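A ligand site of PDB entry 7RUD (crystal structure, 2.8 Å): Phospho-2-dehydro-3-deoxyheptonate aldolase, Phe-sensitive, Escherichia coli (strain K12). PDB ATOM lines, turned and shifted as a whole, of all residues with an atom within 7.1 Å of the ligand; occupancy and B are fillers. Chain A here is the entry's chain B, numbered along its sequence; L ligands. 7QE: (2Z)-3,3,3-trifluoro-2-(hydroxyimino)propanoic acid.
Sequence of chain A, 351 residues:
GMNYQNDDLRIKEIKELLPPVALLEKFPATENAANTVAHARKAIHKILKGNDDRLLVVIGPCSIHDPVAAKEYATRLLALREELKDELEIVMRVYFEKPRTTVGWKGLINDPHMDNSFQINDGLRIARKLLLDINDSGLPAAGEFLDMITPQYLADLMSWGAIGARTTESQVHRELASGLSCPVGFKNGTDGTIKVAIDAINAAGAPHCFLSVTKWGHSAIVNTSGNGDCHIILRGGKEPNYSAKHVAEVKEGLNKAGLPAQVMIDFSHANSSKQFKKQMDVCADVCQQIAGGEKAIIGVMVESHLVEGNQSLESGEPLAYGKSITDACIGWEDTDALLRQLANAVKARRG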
ATOM      1  N   CYS A  62     -19.707   6.310 -29.687  1.00  0.00           N
ATOM      2  CA  CYS A  62     -20.446   5.623 -28.642  1.00  0.00           C
ATOM      3  C   CYS A  62     -21.890   5.431 -29.057  1.00  0.00           C
ATOM      4  O   CYS A  62     -22.426   4.317 -29.015  1.00  0.00           O
ATOM      5  CB  CYS A  62     -20.361   6.428 -27.340  1.00  0.00           C
ATOM      6  SG  CYS A  62     -21.276   5.719 -25.917  1.00  0.00           S
ATOM      7  N   ARG A  93     -18.497   1.713 -35.809  1.00  0.00           N
ATOM      8  CA  ARG A  93     -19.378   1.505 -34.655  1.00  0.00           C
ATOM      9  C   ARG A  93     -20.683   2.254 -34.872  1.00  0.00           C
ATOM     10  O   ARG A  93     -20.772   3.458 -34.618  1.00  0.00           O
ATOM     11  CB  ARG A  93     -18.691   1.979 -33.373  1.00  0.00           C
ATOM     12  CG  ARG A  93     -18.131   0.924 -32.484  1.00  0.00           C
ATOM     13  CD  ARG A  93     -17.762   1.576 -31.178  1.00  0.00           C
ATOM     14  NE  ARG A  93     -18.896   2.282 -30.572  1.00  0.00           N
ATOM     15  CZ  ARG A  93     -19.426   1.973 -29.382  1.00  0.00           C
ATOM     16  NH1 ARG A  93     -20.467   2.660 -28.919  1.00  0.00           N
ATOM     17  NH2 ARG A  93     -18.910   0.980 -28.661  1.00  0.00           N
ATOM     18  N   TYR A  95     -23.837   2.042 -33.247  1.00  0.00           N
ATOM     19  CA  TYR A  95     -24.701   1.593 -32.172  1.00  0.00           C
ATOM     20  C   TYR A  95     -25.946   2.470 -32.152  1.00  0.00           C
ATOM     21  O   TYR A  95     -25.869   3.679 -31.911  1.00  0.00           O
ATOM     22  CB  TYR A  95     -23.970   1.626 -30.833  1.00  0.00           C
ATOM     23  CG  TYR A  95     -22.909   0.545 -30.722  1.00  0.00           C
ATOM     24  CD1 TYR A  95     -22.183   0.149 -31.834  1.00  0.00           C
ATOM     25  CD2 TYR A  95     -22.626  -0.064 -29.492  1.00  0.00           C
ATOM     26  CE1 TYR A  95     -21.221  -0.832 -31.741  1.00  0.00           C
ATOM     27  CE2 TYR A  95     -21.657  -1.033 -29.381  1.00  0.00           C
ATOM     28  CZ  TYR A  95     -20.955  -1.406 -30.508  1.00  0.00           C
ATOM     29  OH  TYR A  95     -19.995  -2.376 -30.427  1.00  0.00           O
ATOM     30  N   LYS A  98     -28.441   2.116 -26.771  1.00  0.00           N
ATOM     31  CA  LYS A  98     -27.566   2.327 -25.616  1.00  0.00           C
ATOM     32  C   LYS A  98     -28.310   2.071 -24.322  1.00  0.00           C
ATOM     33  O   LYS A  98     -29.482   2.479 -24.173  1.00  0.00           O
ATOM     34  CB  LYS A  98     -26.992   3.768 -25.623  1.00  0.00           C
ATOM     35  CG  LYS A  98     -25.822   3.977 -26.604  1.00  0.00           C
ATOM     36  CD  LYS A  98     -24.465   3.437 -26.101  1.00  0.00           C
ATOM     37  CE  LYS A  98     -24.365   1.917 -26.268  1.00  0.00           C
ATOM     38  NZ  LYS A  98     -22.939   1.413 -26.234  1.00  0.00           N
ATOM     39  N   PRO A  99     -27.681   1.376 -23.352  1.00  0.00           N
ATOM     40  CA  PRO A  99     -28.344   1.094 -22.080  1.00  0.00           C
ATOM     41  C   PRO A  99     -27.891   2.041 -20.969  1.00  0.00           C
ATOM     42  O   PRO A  99     -26.707   2.413 -20.933  1.00  0.00           O
ATOM     43  CB  PRO A  99     -27.920  -0.357 -21.806  1.00  0.00           C
ATOM     44  CG  PRO A  99     -26.558  -0.463 -22.380  1.00  0.00           C
ATOM     45  CD  PRO A  99     -26.418   0.606 -23.468  1.00  0.00           C
ATOM     46  N   GLU A 144     -24.507  -3.065 -31.200  1.00  0.00           N
ATOM     47  CA  GLU A 144     -24.869  -3.808 -30.001  1.00  0.00           C
ATOM     48  C   GLU A 144     -26.323  -4.261 -30.084  1.00  0.00           C
ATOM     49  O   GLU A 144     -27.201  -3.480 -30.445  1.00  0.00           O
ATOM     50  CB  GLU A 144     -24.669  -2.975 -28.745  1.00  0.00           C
ATOM     51  CG  GLU A 144     -24.495  -3.818 -27.502  1.00  0.00           C
ATOM     52  CD  GLU A 144     -23.786  -3.059 -26.396  1.00  0.00           C
ATOM     53  OE1 GLU A 144     -24.256  -1.934 -26.079  1.00  0.00           O
ATOM     54  OE2 GLU A 144     -22.775  -3.559 -25.844  1.00  0.00           O
ATOM     55  N   LEU A 146     -29.239  -4.994 -28.000  1.00  0.00           N
ATOM     56  CA  LEU A 146     -29.948  -4.873 -26.728  1.00  0.00           C
ATOM     57  C   LEU A 146     -31.369  -5.406 -26.862  1.00  0.00           C
ATOM     58  O   LEU A 146     -31.674  -6.488 -26.346  1.00  0.00           O
ATOM     59  CB  LEU A 146     -29.976  -3.414 -26.266  1.00  0.00           C
ATOM     60  CG  LEU A 146     -30.085  -3.216 -24.761  1.00  0.00           C
ATOM     61  CD1 LEU A 146     -28.838  -3.771 -24.072  1.00  0.00           C
ATOM     62  CD2 LEU A 146     -30.326  -1.749 -24.404  1.00  0.00           C
ATOM     63  N   ALA A 162     -22.259  -7.036 -30.682  1.00  0.00           N
ATOM     64  CA  ALA A 162     -21.880  -7.158 -29.283  1.00  0.00           C
ATOM     65  C   ALA A 162     -23.114  -7.355 -28.409  1.00  0.00           C
ATOM     66  O   ALA A 162     -24.201  -6.848 -28.717  1.00  0.00           O
ATOM     67  CB  ALA A 162     -21.114  -5.928 -28.808  1.00  0.00           C
ATOM     68  N   ILE A 163     -22.925  -8.098 -27.307  1.00  0.00           N
ATOM     69  CA  ILE A 163     -23.929  -8.223 -26.248  1.00  0.00           C
ATOM     70  C   ILE A 163     -23.411  -7.479 -25.024  1.00  0.00           C
ATOM     71  O   ILE A 163     -22.357  -7.835 -24.472  1.00  0.00           O
ATOM     72  CB  ILE A 163     -24.216  -9.682 -25.891  1.00  0.00           C
ATOM     73  CG1 ILE A 163     -24.873 -10.365 -27.072  1.00  0.00           C
ATOM     74  CG2 ILE A 163     -25.197  -9.704 -24.748  1.00  0.00           C
ATOM     75  CD1 ILE A 163     -26.183  -9.755 -27.377  1.00  0.00           C
ATOM     76  N   GLY A 164     -24.163  -6.481 -24.590  1.00  0.00           N
ATOM     77  CA  GLY A 164     -23.765  -5.616 -23.484  1.00  0.00           C
ATOM     78  C   GLY A 164     -23.151  -6.297 -22.275  1.00  0.00           C
ATOM     79  O   GLY A 164     -23.368  -7.488 -22.025  1.00  0.00           O
ATOM     80  N   ALA A 165     -22.362  -5.532 -21.504  1.00  0.00           N
ATOM     81  CA  ALA A 165     -21.798  -6.093 -20.289  1.00  0.00           C
ATOM     82  C   ALA A 165     -22.901  -6.491 -19.323  1.00  0.00           C
ATOM     83  O   ALA A 165     -22.774  -7.494 -18.610  1.00  0.00           O
ATOM     84  CB  ALA A 165     -20.856  -5.088 -19.612  1.00  0.00           C
ATOM     85  N   ARG A 166     -23.992  -5.740 -19.304  1.00  0.00           N
ATOM     86  CA  ARG A 166     -25.079  -6.003 -18.379  1.00  0.00           C
ATOM     87  C   ARG A 166     -26.071  -7.038 -18.894  1.00  0.00           C
ATOM     88  O   ARG A 166     -26.955  -7.443 -18.132  1.00  0.00           O
ATOM     89  CB  ARG A 166     -25.832  -4.707 -18.034  1.00  0.00           C
ATOM     90  CG  ARG A 166     -24.922  -3.611 -17.527  1.00  0.00           C
ATOM     91  CD  ARG A 166     -25.408  -2.230 -17.965  1.00  0.00           C
ATOM     92  NE  ARG A 166     -24.297  -1.288 -18.179  1.00  0.00           N
ATOM     93  CZ  ARG A 166     -24.396   0.033 -18.029  1.00  0.00           C
ATOM     94  NH1 ARG A 166     -25.554   0.572 -17.663  1.00  0.00           N
ATOM     95  NH2 ARG A 166     -23.333   0.806 -18.248  1.00  0.00           N
ATOM     96  N   THR A 167     -25.959  -7.508 -20.132  1.00  0.00           N
ATOM     97  CA  THR A 167     -26.872  -8.540 -20.615  1.00  0.00           C
ATOM     98  C   THR A 167     -26.177  -9.861 -20.891  1.00  0.00           C
ATOM     99  O   THR A 167     -26.826 -10.799 -21.362  1.00  0.00           O
ATOM    100  CB  THR A 167     -27.617  -8.086 -21.870  1.00  0.00           C
ATOM    101  OG1 THR A 167     -26.728  -7.398 -22.758  1.00  0.00           O
ATOM    102  CG2 THR A 167     -28.817  -7.189 -21.494  1.00  0.00           C
ATOM    103  N   THR A 168     -24.893  -9.969 -20.595  1.00  0.00           N
ATOM    104  CA  THR A 168     -24.155 -11.170 -20.962  1.00  0.00           C
ATOM    105  C   THR A 168     -24.644 -12.398 -20.218  1.00  0.00           C
ATOM    106  O   THR A 168     -24.487 -13.522 -20.718  1.00  0.00           O
ATOM    107  CB  THR A 168     -22.652 -10.952 -20.738  1.00  0.00           C
ATOM    108  OG1 THR A 168     -22.182  -9.900 -21.614  1.00  0.00           O
ATOM    109  CG2 THR A 168     -21.875 -12.244 -21.014  1.00  0.00           C
ATOM    110  N   LYS A 187     -19.049  -9.258 -23.736  1.00  0.00           N
ATOM    111  CA  LYS A 187     -18.234  -8.558 -22.748  1.00  0.00           C
ATOM    112  C   LYS A 187     -18.201  -9.322 -21.416  1.00  0.00           C
ATOM    113  O   LYS A 187     -19.102 -10.093 -21.098  1.00  0.00           O
ATOM    114  CB  LYS A 187     -18.786  -7.153 -22.512  1.00  0.00           C
ATOM    115  CG  LYS A 187     -18.619  -6.230 -23.671  1.00  0.00           C
ATOM    116  CD  LYS A 187     -19.403  -4.947 -23.462  1.00  0.00           C
ATOM    117  CE  LYS A 187     -18.697  -3.807 -24.172  1.00  0.00           C
ATOM    118  NZ  LYS A 187     -17.613  -4.390 -25.016  1.00  0.00           N
ATOM    119  N   ASN A 188     -17.139  -9.095 -20.632  1.00  0.00           N
ATOM    120  CA  ASN A 188     -17.062  -9.672 -19.286  1.00  0.00           C
ATOM    121  C   ASN A 188     -18.027  -8.938 -18.359  1.00  0.00           C
ATOM    122  O   ASN A 188     -18.593  -7.885 -18.694  1.00  0.00           O
ATOM    123  CB  ASN A 188     -15.633  -9.624 -18.731  1.00  0.00           C
ATOM    124  CG  ASN A 188     -14.997  -8.244 -18.826  1.00  0.00           C
ATOM    125  OD1 ASN A 188     -14.178  -7.969 -19.710  1.00  0.00           O
ATOM    126  ND2 ASN A 188     -15.386  -7.363 -17.910  1.00  0.00           N
ATOM    127  N   THR A 190     -19.628  -6.594 -15.636  1.00  0.00           N
ATOM    128  CA  THR A 190     -19.346  -5.256 -15.133  1.00  0.00           C
ATOM    129  C   THR A 190     -18.432  -5.223 -13.916  1.00  0.00           C
ATOM    130  O   THR A 190     -17.771  -4.211 -13.677  1.00  0.00           O
ATOM    131  CB  THR A 190     -20.651  -4.555 -14.766  1.00  0.00           C
ATOM    132  OG1 THR A 190     -21.395  -5.375 -13.859  1.00  0.00           O
ATOM    133  CG2 THR A 190     -21.479  -4.297 -16.020  1.00  0.00           C
ATOM    134  N   ILE A 233     -15.205 -10.362 -25.146  1.00  0.00           N
ATOM    135  CA  ILE A 233     -14.748  -8.979 -25.148  1.00  0.00           C
ATOM    136  C   ILE A 233     -14.271  -8.619 -23.738  1.00  0.00           C
ATOM    137  O   ILE A 233     -15.027  -8.760 -22.766  1.00  0.00           O
ATOM    138  CB  ILE A 233     -15.856  -8.002 -25.571  1.00  0.00           C
ATOM    139  CG1 ILE A 233     -16.345  -8.267 -26.981  1.00  0.00           C
ATOM    140  CG2 ILE A 233     -15.361  -6.578 -25.460  1.00  0.00           C
ATOM    141  CD1 ILE A 233     -17.370  -7.260 -27.417  1.00  0.00           C
ATOM    142  N   ARG A 235     -13.379  -5.720 -21.132  1.00  0.00           N
ATOM    143  CA  ARG A 235     -13.831  -4.330 -21.044  1.00  0.00           C
ATOM    144  C   ARG A 235     -13.547  -3.724 -19.684  1.00  0.00           C
ATOM    145  O   ARG A 235     -14.053  -2.625 -19.398  1.00  0.00           O
ATOM    146  CB  ARG A 235     -15.331  -4.223 -21.368  1.00  0.00           C
ATOM    147  CG  ARG A 235     -16.249  -5.020 -20.435  1.00  0.00           C
ATOM    148  CD  ARG A 235     -17.347  -4.123 -19.895  1.00  0.00           C
ATOM    149  NE  ARG A 235     -17.036  -3.555 -18.581  1.00  0.00           N
ATOM    150  CZ  ARG A 235     -17.707  -2.540 -18.033  1.00  0.00           C
ATOM    151  NH1 ARG A 235     -17.357  -2.086 -16.841  1.00  0.00           N
ATOM    152  NH2 ARG A 235     -18.722  -1.977 -18.670  1.00  0.00           N
ATOM    153  N   ASP A 266     -11.361  -4.305 -25.262  1.00  0.00           N
ATOM    154  CA  ASP A 266     -11.884  -2.958 -25.313  1.00  0.00           C
ATOM    155  C   ASP A 266     -10.820  -2.002 -24.780  1.00  0.00           C
ATOM    156  O   ASP A 266      -9.921  -2.398 -24.030  1.00  0.00           O
ATOM    157  CB  ASP A 266     -13.176  -2.886 -24.497  1.00  0.00           C
ATOM    158  CG  ASP A 266     -14.059  -1.705 -24.859  1.00  0.00           C
ATOM    159  OD1 ASP A 266     -13.585  -0.820 -25.602  1.00  0.00           O
ATOM    160  OD2 ASP A 266     -15.210  -1.644 -24.366  1.00  0.00           O
ATOM    161  N   SER A 268     -12.082   1.405 -24.117  1.00  0.00           N
ATOM    162  CA  SER A 268     -12.888   2.434 -23.483  1.00  0.00           C
ATOM    163  C   SER A 268     -13.464   1.879 -22.172  1.00  0.00           C
ATOM    164  O   SER A 268     -12.978   0.859 -21.669  1.00  0.00           O
ATOM    165  CB  SER A 268     -13.982   2.904 -24.462  1.00  0.00           C
ATOM    166  OG  SER A 268     -14.858   3.848 -23.872  1.00  0.00           O
ATOM    167  N   HIS A 269     -14.470   2.550 -21.607  1.00  0.00           N
ATOM    168  CA  HIS A 269     -15.266   2.049 -20.467  1.00  0.00           C
ATOM    169  C   HIS A 269     -14.340   1.746 -19.280  1.00  0.00           C
ATOM    170  O   HIS A 269     -13.560   2.622 -18.882  1.00  0.00           O
ATOM    171  CB  HIS A 269     -16.132   0.884 -20.951  1.00  0.00           C
ATOM    172  CG  HIS A 269     -16.801   1.136 -22.272  1.00  0.00           C
ATOM    173  ND1 HIS A 269     -16.720   0.242 -23.322  1.00  0.00           N
ATOM    174  CD2 HIS A 269     -17.569   2.167 -22.701  1.00  0.00           C
ATOM    175  CE1 HIS A 269     -17.400   0.717 -24.356  1.00  0.00           C
ATOM    176  NE2 HIS A 269     -17.926   1.877 -23.998  1.00  0.00           N
ATOM    177  N   ALA A 270     -14.395   0.554 -18.685  1.00  0.00           N
ATOM    178  CA  ALA A 270     -13.649   0.325 -17.444  1.00  0.00           C
ATOM    179  C   ALA A 270     -12.155   0.263 -17.713  1.00  0.00           C
ATOM    180  O   ALA A 270     -11.340   0.688 -16.871  1.00  0.00           O
ATOM    181  CB  ALA A 270     -14.143  -0.946 -16.736  1.00  0.00           C
ATOM    182  N   MET A 301     -11.558  -2.658 -29.648  1.00  0.00           N
ATOM    183  CA  MET A 301     -12.659  -1.740 -29.891  1.00  0.00           C
ATOM    184  C   MET A 301     -12.353  -0.432 -29.202  1.00  0.00           C
ATOM    185  O   MET A 301     -11.623  -0.398 -28.217  1.00  0.00           O
ATOM    186  CB  MET A 301     -13.976  -2.350 -29.419  1.00  0.00           C
ATOM    187  CG  MET A 301     -15.136  -1.383 -29.208  1.00  0.00           C
ATOM    188  SD  MET A 301     -16.333  -2.137 -28.051  1.00  0.00           S
ATOM    189  CE  MET A 301     -16.123  -3.883 -28.435  1.00  0.00           C
ATOM    190  N   GLU A 303     -13.763   3.863 -28.762  1.00  0.00           N
ATOM    191  CA  GLU A 303     -14.897   4.791 -28.827  1.00  0.00           C
ATOM    192  C   GLU A 303     -14.389   6.093 -29.442  1.00  0.00           C
ATOM    193  O   GLU A 303     -13.693   6.879 -28.773  1.00  0.00           O
ATOM    194  CB  GLU A 303     -15.524   4.996 -27.445  1.00  0.00           C
ATOM    195  CG  GLU A 303     -16.243   3.765 -26.889  1.00  0.00           C
ATOM    196  CD  GLU A 303     -17.330   4.082 -25.849  1.00  0.00           C
ATOM    197  OE1 GLU A 303     -17.083   4.877 -24.896  1.00  0.00           O
ATOM    198  OE2 GLU A 303     -18.445   3.518 -25.972  1.00  0.00           O
ATOM    199  N   ASP A 327     -21.313   8.442 -23.730  1.00  0.00           N
ATOM    200  CA  ASP A 327     -19.898   8.251 -23.416  1.00  0.00           C
ATOM    201  C   ASP A 327     -19.045   9.196 -24.254  1.00  0.00           C
ATOM    202  O   ASP A 327     -19.425   9.591 -25.371  1.00  0.00           O
ATOM    203  CB  ASP A 327     -19.477   6.796 -23.677  1.00  0.00           C
ATOM    204  CG  ASP A 327     -19.568   5.923 -22.421  1.00  0.00           C
ATOM    205  OD1 ASP A 327     -20.263   6.339 -21.467  1.00  0.00           O
ATOM    206  OD2 ASP A 327     -18.930   4.845 -22.384  1.00  0.00           O
HETATM  207  C2  7QE L   1     -21.016  -1.417 -22.838  1.00  0.00           C
HETATM  208  N1  7QE L   1     -21.149  -1.066 -24.098  1.00  0.00           N
HETATM  209  O2  7QE L   1     -22.849  -2.004 -21.749  1.00  0.00           O
HETATM  210  C1  7QE L   1     -21.945  -2.298 -22.563  1.00  0.00           C
HETATM  211  C3  7QE L   1     -20.012  -1.024 -21.761  1.00  0.00           C
HETATM  212  F1  7QE L   1     -18.977  -1.878 -21.695  1.00  0.00           F
HETATM  213  F2  7QE L   1     -20.531  -0.953 -20.530  1.00  0.00           F
HETATM  214  F3  7QE L   1     -19.535   0.185 -21.932  1.00  0.00           F
HETATM  215  O1  7QE L   1     -21.829  -3.387 -23.178  1.00  0.00           O
HETATM  216  O3  7QE L   1     -20.327  -0.132 -24.753  1.00  0.00           O
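The side-chain amino group of Lys 98 sits at hydrogen-bond distance from an oxygen (O3) of the ligand (3.4 Å).
A ring nitrogen (NE2) of His 269 sits close to an oxygen (O3) of the ligand (3.2 Å).
The side-chain carboxylate of Glu 144 sits close to an oxygen (O1) of the ligand (2.8 Å).
NE of Arg 166 lies within salt-bridge range of O2 of the ligand.
O1 of the ligand is in hydrogen-bond range of N of Ala 165, 2.8 Å away.
The side-chain carboxylate (OE2) of Glu 144 sits close to the backbone NH (N) of Gly 164.
ND1 of His 269 sits at hydrogen-bond distance from OD2 of Asp 266.
The side-chain hydroxyl (OG1) of Thr 168 sits at hydrogen-bond distance from the backbone carbonyl oxygen (O) of Lys 187, at 3.1 Å.
The side-chain hydroxyl (OG1) of Thr 167 is in hydrogen-bond range of the backbone NH (N) of Gly 164 (3.3 Å).
NZ of Lys 187 is in salt-bridge range of OD2 of Asp 266, 3.7 Å away.
NZ of Lys 98 is in salt-bridge range of OE1 of Glu 144.
OE2 of Glu 303 sits at hydrogen-bond distance from NE2 of His 269.
The backbone NH (N) of Arg 235 is in hydrogen-bond range of the side-chain amide oxygen (OD1) of Asn 188, at 2.8 Å.
The guanidinium group of Arg 235 lies close to a fluorine (F2) of the ligand (2.8 Å).
Residues that only touch the ligand: Lys 187 (2.9 Å) and Gly 164 (3.0 Å).
Hydrophobic or aromatic side chains within 4 Å of the ligand: His 269.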
